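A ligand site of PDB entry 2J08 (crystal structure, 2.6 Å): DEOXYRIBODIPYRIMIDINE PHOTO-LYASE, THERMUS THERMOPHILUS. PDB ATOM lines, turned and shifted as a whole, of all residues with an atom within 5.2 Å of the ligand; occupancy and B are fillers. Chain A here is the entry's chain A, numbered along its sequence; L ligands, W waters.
O4 of the ligand sits at hydrogen-bond distance from NH1 of Arg 104, 2.5 Å away.
A nitrogen (N2) of the ligand lies within hydrogen-bond range of the backbone carbonyl oxygen of Val 34.
The backbone NH (N) of Gly 10 is in hydrogen-bond range of an oxygen (O5) of the ligand (3.1 Å).
ND2 of Asn 39 lies close to N1 of the ligand, at 3.4 Å.
N of Asp 36 lies within hydrogen-bond range of O2 of the ligand, at 3.2 Å.
The side-chain carboxylate (OD2) of Asp 36 sits at hydrogen-bond distance from the side-chain hydroxyl (OH) of Tyr 100 (2.6 Å).
OG of Ser 96 lies within hydrogen-bond range of OG1 of Thr 98, at 3.3 Å.
The backbone carbonyl oxygen (O) of Gly 342 lies within hydrogen-bond range of the guanidinium group (NH2) of Arg 46.
The side-chain carboxylate of Asp 11 sits at hydrogen-bond distance from the backbone NH of Arg 9 (3.1 Å).
NH2 of Arg 9 sits at hydrogen-bond distance from O of Leu 94 (2.7 Å).
N of Asp 11 sits at hydrogen-bond distance from O of Leu 218, 3.2 Å away.
The guanidinium group (NH1) of Arg 46 lies within hydrogen-bond range of the side-chain hydroxyl (OG1) of Thr 42 (2.8 Å).
Residues that only touch the ligand: Phe 50, Ser 96, Gly 342, Arg 9, Leu 40, Leu 35, Leu 218 and Arg 46.
Hydrophobic or aromatic side chains that line the ligand: Leu 40, Phe 50 and Leu 218.
13 residues have an atom within 4 Å of the ligand: Arg 9, Gly 10, Val 34, Leu 35, Asp 36, Asn 39, Leu 40, Arg 46, Phe 50, Ser 96, Arg 104, Leu 218 and Gly 342.
Water W2 lies within hydrogen-bond range of an oxygen (O1) of the ligand (2.5 Å), the backbone carbonyl oxygen of His 8 (2.8 Å), the indole nitrogen of Trp 7 (2.9 Å) and the backbone NH of Val 34 (3.0 Å).
Water W3 lies within hydrogen-bond range of O6 of the ligand (2.9 Å), O of Leu 94 (3.0 Å), OD1 of Asp 11 (3.2 Å) and NE of Arg 9 (3.3 Å).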
ATOM      1  N   TRP A   7     -27.677  25.579  20.484  1.00  0.00           N
ATOM      2  CA  TRP A   7     -26.789  25.188  19.443  1.00  0.00           C
ATOM      3  C   TRP A   7     -25.320  25.612  19.759  1.00  0.00           C
ATOM      4  O   TRP A   7     -24.958  26.794  19.804  1.00  0.00           O
ATOM      5  CB  TRP A   7     -27.350  25.753  18.113  1.00  0.00           C
ATOM      6  CG  TRP A   7     -26.595  25.411  16.815  1.00  0.00           C
ATOM      7  CD1 TRP A   7     -25.677  24.377  16.606  1.00  0.00           C
ATOM      8  CD2 TRP A   7     -26.592  26.205  15.606  1.00  0.00           C
ATOM      9  NE1 TRP A   7     -25.158  24.464  15.301  1.00  0.00           N
ATOM     10  CE2 TRP A   7     -25.735  25.543  14.666  1.00  0.00           C
ATOM     11  CE3 TRP A   7     -27.404  27.237  15.138  1.00  0.00           C
ATOM     12  CZ2 TRP A   7     -25.573  25.997  13.337  1.00  0.00           C
ATOM     13  CZ3 TRP A   7     -27.159  27.759  13.778  1.00  0.00           C
ATOM     14  CH2 TRP A   7     -26.261  27.133  12.928  1.00  0.00           C
ATOM     15  N   HIS A   8     -24.474  24.608  20.074  1.00  0.00           N
ATOM     16  CA  HIS A   8     -23.061  24.846  20.414  1.00  0.00           C
ATOM     17  C   HIS A   8     -22.334  24.731  19.101  1.00  0.00           C
ATOM     18  O   HIS A   8     -22.402  23.679  18.474  1.00  0.00           O
ATOM     19  CB  HIS A   8     -22.496  23.755  21.333  1.00  0.00           C
ATOM     20  CG  HIS A   8     -23.019  23.801  22.727  1.00  0.00           C
ATOM     21  ND1 HIS A   8     -22.333  24.414  23.753  1.00  0.00           N
ATOM     22  CD2 HIS A   8     -24.163  23.317  23.276  1.00  0.00           C
ATOM     23  CE1 HIS A   8     -23.056  24.371  24.856  1.00  0.00           C
ATOM     24  NE2 HIS A   8     -24.155  23.663  24.607  1.00  0.00           N
ATOM     25  N   ARG A   9     -21.536  25.731  18.742  1.00  0.00           N
ATOM     26  CA  ARG A   9     -20.599  25.564  17.653  1.00  0.00           C
ATOM     27  C   ARG A   9     -19.189  25.509  18.263  1.00  0.00           C
ATOM     28  O   ARG A   9     -18.871  24.517  18.943  1.00  0.00           O
ATOM     29  CB  ARG A   9     -20.746  26.693  16.645  1.00  0.00           C
ATOM     30  CG  ARG A   9     -22.064  26.704  15.972  1.00  0.00           C
ATOM     31  CD  ARG A   9     -23.229  27.332  16.782  1.00  0.00           C
ATOM     32  NE  ARG A   9     -23.163  28.793  16.692  1.00  0.00           N
ATOM     33  CZ  ARG A   9     -23.644  29.528  15.685  1.00  0.00           C
ATOM     34  NH1 ARG A   9     -24.285  28.969  14.657  1.00  0.00           N
ATOM     35  NH2 ARG A   9     -23.353  30.821  15.646  1.00  0.00           N
ATOM     36  N   GLY A  10     -18.298  26.448  17.905  1.00  0.00           N
ATOM     37  CA  GLY A  10     -16.965  26.465  18.501  1.00  0.00           C
ATOM     38  C   GLY A  10     -17.092  27.053  19.908  1.00  0.00           C
ATOM     39  O   GLY A  10     -16.572  28.148  20.207  1.00  0.00           O
ATOM     40  N   ASP A  11     -17.858  26.364  20.759  1.00  0.00           N
ATOM     41  CA  ASP A  11     -18.008  26.768  22.152  1.00  0.00           C
ATOM     42  C   ASP A  11     -18.457  25.574  22.909  1.00  0.00           C
ATOM     43  O   ASP A  11     -19.626  25.463  23.275  1.00  0.00           O
ATOM     44  CB  ASP A  11     -18.976  27.927  22.323  1.00  0.00           C
ATOM     45  CG  ASP A  11     -20.036  27.979  21.229  1.00  0.00           C
ATOM     46  OD1 ASP A  11     -19.857  28.768  20.240  1.00  0.00           O
ATOM     47  OD2 ASP A  11     -21.058  27.284  21.435  1.00  0.00           O
ATOM     48  N   VAL A  33     -25.217  19.798  18.755  1.00  0.00           N
ATOM     49  CA  VAL A  33     -24.156  20.020  17.821  1.00  0.00           C
ATOM     50  C   VAL A  33     -24.477  19.421  16.448  1.00  0.00           C
ATOM     51  O   VAL A  33     -25.040  18.318  16.343  1.00  0.00           O
ATOM     52  CB  VAL A  33     -22.874  19.367  18.351  1.00  0.00           C
ATOM     53  CG1 VAL A  33     -21.796  19.312  17.196  1.00  0.00           C
ATOM     54  CG2 VAL A  33     -22.399  20.057  19.587  1.00  0.00           C
ATOM     55  N   VAL A  34     -23.964  20.080  15.424  1.00  0.00           N
ATOM     56  CA  VAL A  34     -24.058  19.583  14.047  1.00  0.00           C
ATOM     57  C   VAL A  34     -22.625  19.463  13.560  1.00  0.00           C
ATOM     58  O   VAL A  34     -21.919  20.497  13.566  1.00  0.00           O
ATOM     59  CB  VAL A  34     -24.678  20.656  13.070  1.00  0.00           C
ATOM     60  CG1 VAL A  34     -24.564  20.177  11.638  1.00  0.00           C
ATOM     61  CG2 VAL A  34     -26.170  20.996  13.416  1.00  0.00           C
ATOM     62  N   LEU A  35     -22.265  18.265  13.057  1.00  0.00           N
ATOM     63  CA  LEU A  35     -20.976  17.957  12.460  1.00  0.00           C
ATOM     64  C   LEU A  35     -21.132  18.356  10.985  1.00  0.00           C
ATOM     65  O   LEU A  35     -21.873  17.735  10.187  1.00  0.00           O
ATOM     66  CB  LEU A  35     -20.636  16.460  12.688  1.00  0.00           C
ATOM     67  CG  LEU A  35     -20.950  15.915  14.139  1.00  0.00           C
ATOM     68  CD1 LEU A  35     -20.508  14.479  14.425  1.00  0.00           C
ATOM     69  CD2 LEU A  35     -20.346  16.796  15.298  1.00  0.00           C
ATOM     70  N   ASP A  36     -20.538  19.487  10.651  1.00  0.00           N
ATOM     71  CA  ASP A  36     -20.801  20.196   9.448  1.00  0.00           C
ATOM     72  C   ASP A  36     -19.712  19.887   8.499  1.00  0.00           C
ATOM     73  O   ASP A  36     -18.535  20.201   8.781  1.00  0.00           O
ATOM     74  CB  ASP A  36     -20.736  21.681   9.793  1.00  0.00           C
ATOM     75  CG  ASP A  36     -21.098  22.613   8.628  1.00  0.00           C
ATOM     76  OD1 ASP A  36     -20.922  22.287   7.395  1.00  0.00           O
ATOM     77  OD2 ASP A  36     -21.222  23.788   8.960  1.00  0.00           O
ATOM     78  N   ASN A  39     -16.791  22.317   8.104  1.00  0.00           N
ATOM     79  CA  ASN A  39     -15.656  22.408   9.077  1.00  0.00           C
ATOM     80  C   ASN A  39     -14.904  21.085   9.121  1.00  0.00           C
ATOM     81  O   ASN A  39     -13.819  21.036   9.646  1.00  0.00           O
ATOM     82  CB  ASN A  39     -16.168  22.788  10.503  1.00  0.00           C
ATOM     83  CG  ASN A  39     -16.978  24.057  10.495  1.00  0.00           C
ATOM     84  OD1 ASN A  39     -16.636  24.992   9.820  1.00  0.00           O
ATOM     85  ND2 ASN A  39     -18.117  24.070  11.164  1.00  0.00           N
ATOM     86  N   LEU A  40     -15.550  19.975   8.753  1.00  0.00           N
ATOM     87  CA  LEU A  40     -14.904  18.710   9.044  1.00  0.00           C
ATOM     88  C   LEU A  40     -14.295  17.967   7.897  1.00  0.00           C
ATOM     89  O   LEU A  40     -13.837  16.851   8.086  1.00  0.00           O
ATOM     90  CB  LEU A  40     -15.792  17.757   9.839  1.00  0.00           C
ATOM     91  CG  LEU A  40     -16.336  18.072  11.233  1.00  0.00           C
ATOM     92  CD1 LEU A  40     -17.359  17.008  11.503  1.00  0.00           C
ATOM     93  CD2 LEU A  40     -15.259  18.134  12.377  1.00  0.00           C
ATOM     94  N   THR A  42     -11.292  18.137   6.728  1.00  0.00           N
ATOM     95  CA  THR A  42      -9.974  18.719   7.090  1.00  0.00           C
ATOM     96  C   THR A  42      -9.117  17.550   7.539  1.00  0.00           C
ATOM     97  O   THR A  42      -9.505  16.418   7.296  1.00  0.00           O
ATOM     98  CB  THR A  42     -10.136  19.726   8.241  1.00  0.00           C
ATOM     99  OG1 THR A  42      -8.882  20.347   8.471  1.00  0.00           O
ATOM    100  CG2 THR A  42     -10.627  19.059   9.561  1.00  0.00           C
ATOM    101  N   ARG A  46      -7.701  17.001  13.242  1.00  0.00           N
ATOM    102  CA  ARG A  46      -8.572  18.067  13.651  1.00  0.00           C
ATOM    103  C   ARG A  46      -9.996  17.538  13.687  1.00  0.00           C
ATOM    104  O   ARG A  46     -10.733  17.929  14.578  1.00  0.00           O
ATOM    105  CB  ARG A  46      -8.489  19.249  12.704  1.00  0.00           C
ATOM    106  CG  ARG A  46      -7.146  19.787  12.577  1.00  0.00           C
ATOM    107  CD  ARG A  46      -7.102  20.729  11.472  1.00  0.00           C
ATOM    108  NE  ARG A  46      -7.378  22.016  11.979  1.00  0.00           N
ATOM    109  CZ  ARG A  46      -8.105  22.899  11.326  1.00  0.00           C
ATOM    110  NH1 ARG A  46      -8.578  22.533  10.140  1.00  0.00           N
ATOM    111  NH2 ARG A  46      -8.426  24.092  11.863  1.00  0.00           N
ATOM    112  N   PHE A  50     -11.961  17.820  17.273  1.00  0.00           N
ATOM    113  CA  PHE A  50     -13.339  18.374  17.374  1.00  0.00           C
ATOM    114  C   PHE A  50     -14.307  17.294  17.917  1.00  0.00           C
ATOM    115  O   PHE A  50     -14.919  17.471  18.988  1.00  0.00           O
ATOM    116  CB  PHE A  50     -13.816  19.100  16.103  1.00  0.00           C
ATOM    117  CG  PHE A  50     -15.205  19.785  16.236  1.00  0.00           C
ATOM    118  CD1 PHE A  50     -15.332  21.049  16.822  1.00  0.00           C
ATOM    119  CD2 PHE A  50     -16.378  19.143  15.760  1.00  0.00           C
ATOM    120  CE1 PHE A  50     -16.580  21.608  17.013  1.00  0.00           C
ATOM    121  CE2 PHE A  50     -17.632  19.664  16.023  1.00  0.00           C
ATOM    122  CZ  PHE A  50     -17.741  20.908  16.548  1.00  0.00           C
ATOM    123  N   LEU A  94     -24.113  31.592  19.887  1.00  0.00           N
ATOM    124  CA  LEU A  94     -23.185  32.722  20.031  1.00  0.00           C
ATOM    125  C   LEU A  94     -22.935  33.303  18.649  1.00  0.00           C
ATOM    126  O   LEU A  94     -22.708  32.548  17.660  1.00  0.00           O
ATOM    127  CB  LEU A  94     -21.867  32.246  20.628  1.00  0.00           C
ATOM    128  CG  LEU A  94     -22.075  31.731  22.072  1.00  0.00           C
ATOM    129  CD1 LEU A  94     -20.722  31.269  22.717  1.00  0.00           C
ATOM    130  CD2 LEU A  94     -22.866  32.682  23.046  1.00  0.00           C
ATOM    131  N   SER A  96     -21.424  34.784  15.276  1.00  0.00           N
ATOM    132  CA  SER A  96     -20.128  34.536  14.643  1.00  0.00           C
ATOM    133  C   SER A  96     -19.912  35.629  13.631  1.00  0.00           C
ATOM    134  O   SER A  96     -20.760  35.890  12.758  1.00  0.00           O
ATOM    135  CB  SER A  96     -20.144  33.174  13.923  1.00  0.00           C
ATOM    136  OG  SER A  96     -18.947  32.944  13.210  1.00  0.00           O
ATOM    137  N   THR A  98     -17.586  35.825  11.276  1.00  0.00           N
ATOM    138  CA  THR A  98     -16.827  35.358  10.138  1.00  0.00           C
ATOM    139  C   THR A  98     -17.690  35.083   8.908  1.00  0.00           C
ATOM    140  O   THR A  98     -18.941  34.985   8.983  1.00  0.00           O
ATOM    141  CB  THR A  98     -16.148  34.057  10.471  1.00  0.00           C
ATOM    142  OG1 THR A  98     -17.139  33.026  10.451  1.00  0.00           O
ATOM    143  CG2 THR A  98     -15.496  34.166  11.837  1.00  0.00           C
ATOM    144  N   TYR A 100     -18.161  32.714   7.032  1.00  0.00           N
ATOM    145  CA  TYR A 100     -18.953  31.468   6.925  1.00  0.00           C
ATOM    146  C   TYR A 100     -20.032  31.449   7.988  1.00  0.00           C
ATOM    147  O   TYR A 100     -21.181  31.007   7.699  1.00  0.00           O
ATOM    148  CB  TYR A 100     -18.120  30.185   7.029  1.00  0.00           C
ATOM    149  CG  TYR A 100     -19.011  28.963   7.043  1.00  0.00           C
ATOM    150  CD1 TYR A 100     -19.772  28.601   5.908  1.00  0.00           C
ATOM    151  CD2 TYR A 100     -19.123  28.166   8.171  1.00  0.00           C
ATOM    152  CE1 TYR A 100     -20.619  27.403   5.899  1.00  0.00           C
ATOM    153  CE2 TYR A 100     -19.922  26.993   8.161  1.00  0.00           C
ATOM    154  CZ  TYR A 100     -20.731  26.647   7.048  1.00  0.00           C
ATOM    155  OH  TYR A 100     -21.594  25.510   7.106  1.00  0.00           O
ATOM    156  N   GLY A 101     -19.654  31.838   9.216  1.00  0.00           N
ATOM    157  CA  GLY A 101     -20.574  32.206  10.246  1.00  0.00           C
ATOM    158  C   GLY A 101     -21.756  32.990   9.728  1.00  0.00           C
ATOM    159  O   GLY A 101     -22.881  32.553   9.821  1.00  0.00           O
ATOM    160  N   ARG A 104     -23.766  30.786   7.014  1.00  0.00           N
ATOM    161  CA  ARG A 104     -24.520  29.636   7.568  1.00  0.00           C
ATOM    162  C   ARG A 104     -25.706  30.164   8.442  1.00  0.00           C
ATOM    163  O   ARG A 104     -26.856  29.755   8.237  1.00  0.00           O
ATOM    164  CB  ARG A 104     -23.571  28.760   8.418  1.00  0.00           C
ATOM    165  CG  ARG A 104     -24.274  27.944   9.474  1.00  0.00           C
ATOM    166  CD  ARG A 104     -23.344  27.478  10.607  1.00  0.00           C
ATOM    167  NE  ARG A 104     -23.009  28.595  11.478  1.00  0.00           N
ATOM    168  CZ  ARG A 104     -21.831  28.738  12.064  1.00  0.00           C
ATOM    169  NH1 ARG A 104     -20.963  27.743  11.975  1.00  0.00           N
ATOM    170  NH2 ARG A 104     -21.520  29.837  12.768  1.00  0.00           N
ATOM    171  N   ALA A 217      -9.380  27.173  20.814  1.00  0.00           N
ATOM    172  CA  ALA A 217      -9.780  27.098  19.420  1.00  0.00           C
ATOM    173  C   ALA A 217     -11.194  26.533  19.215  1.00  0.00           C
ATOM    174  O   ALA A 217     -11.910  26.976  18.300  1.00  0.00           O
ATOM    175  CB  ALA A 217      -8.785  26.255  18.696  1.00  0.00           C
ATOM    176  N   LEU A 218     -11.581  25.548  20.042  1.00  0.00           N
ATOM    177  CA  LEU A 218     -12.934  25.035  20.024  1.00  0.00           C
ATOM    178  C   LEU A 218     -13.817  25.738  21.067  1.00  0.00           C
ATOM    179  O   LEU A 218     -14.901  25.233  21.410  1.00  0.00           O
ATOM    180  CB  LEU A 218     -12.896  23.571  20.336  1.00  0.00           C
ATOM    181  CG  LEU A 218     -12.003  22.839  19.302  1.00  0.00           C
ATOM    182  CD1 LEU A 218     -11.969  21.355  19.607  1.00  0.00           C
ATOM    183  CD2 LEU A 218     -12.448  23.008  17.803  1.00  0.00           C
ATOM    184  N   GLY A 342      -5.400  25.086  15.150  1.00  0.00           N
ATOM    185  CA  GLY A 342      -5.381  25.851  13.894  1.00  0.00           C
ATOM    186  C   GLY A 342      -6.656  26.637  13.720  1.00  0.00           C
ATOM    187  O   GLY A 342      -7.724  26.184  14.072  1.00  0.00           O
ATOM    188  N   ASP A 343      -6.508  27.918  13.439  1.00  0.00           N
ATOM    189  CA  ASP A 343      -7.621  28.831  13.593  1.00  0.00           C
ATOM    190  C   ASP A 343      -7.396  29.853  12.520  1.00  0.00           C
ATOM    191  O   ASP A 343      -6.376  30.513  12.508  1.00  0.00           O
ATOM    192  CB  ASP A 343      -7.577  29.494  14.953  1.00  0.00           C
ATOM    193  CG  ASP A 343      -8.667  30.522  15.165  1.00  0.00           C
ATOM    194  OD1 ASP A 343      -8.814  31.455  14.340  1.00  0.00           O
ATOM    195  OD2 ASP A 343      -9.286  30.478  16.240  1.00  0.00           O
HETATM  196  N1  LIG L   1     -18.609  24.035  14.566  1.00  0.00           N
HETATM  197  C1  LIG L   1     -19.727  23.283  14.237  1.00  0.00           C
HETATM  198  O1  LIG L   1     -20.847  23.778  14.527  1.00  0.00           O
HETATM  199  N2  LIG L   1     -19.670  22.053  13.661  1.00  0.00           N
HETATM  200  C2  LIG L   1     -18.481  21.505  13.375  1.00  0.00           C
HETATM  201  O2  LIG L   1     -18.406  20.340  12.879  1.00  0.00           O
HETATM  202  C3  LIG L   1     -17.257  22.287  13.698  1.00  0.00           C
HETATM  203  N3  LIG L   1     -16.046  21.775  13.529  1.00  0.00           N
HETATM  204  C4  LIG L   1     -14.900  22.448  13.821  1.00  0.00           C
HETATM  205  C5  LIG L   1     -13.688  21.842  13.561  1.00  0.00           C
HETATM  206  C6  LIG L   1     -12.516  22.517  13.821  1.00  0.00           C
HETATM  207  C7  LIG L   1     -11.176  21.834  13.574  1.00  0.00           C
HETATM  208  C8  LIG L   1     -12.604  23.923  14.339  1.00  0.00           C
HETATM  209  C9  LIG L   1     -13.820  24.547  14.562  1.00  0.00           C
HETATM  210  C10 LIG L   1     -14.961  23.844  14.257  1.00  0.00           C
HETATM  211  N4  LIG L   1     -16.220  24.367  14.597  1.00  0.00           N
HETATM  212  C11 LIG L   1     -17.372  23.651  14.227  1.00  0.00           C
HETATM  213  C12 LIG L   1     -16.231  25.810  14.804  1.00  0.00           C
HETATM  214  C13 LIG L   1     -16.571  26.510  13.547  1.00  0.00           C
HETATM  215  O3  LIG L   1     -15.339  27.073  13.025  1.00  0.00           O
HETATM  216  C14 LIG L   1     -17.722  27.475  13.874  1.00  0.00           C
HETATM  217  O4  LIG L   1     -18.571  27.799  12.770  1.00  0.00           O
HETATM  218  C15 LIG L   1     -17.290  28.802  14.427  1.00  0.00           C
HETATM  219  O5  LIG L   1     -17.417  28.585  15.842  1.00  0.00           O
HETATM  220  C16 LIG L   1     -18.386  29.790  14.061  1.00  0.00           C
HETATM  221  I1  LIG L   1     -10.800  24.982  14.677  1.00  0.00           I
HETATM  222  O6  LIG L   1     -19.269  29.763  15.218  1.00  0.00           O
HETATM  223  O   HOH W   1     -22.915  23.806  12.584  1.00  0.00           O
HETATM  224  O   HOH W   2     -22.790  22.841  15.852  1.00  0.00           O
HETATM  225  O   HOH W   3     -20.547  30.475  17.675  1.00  0.00           O
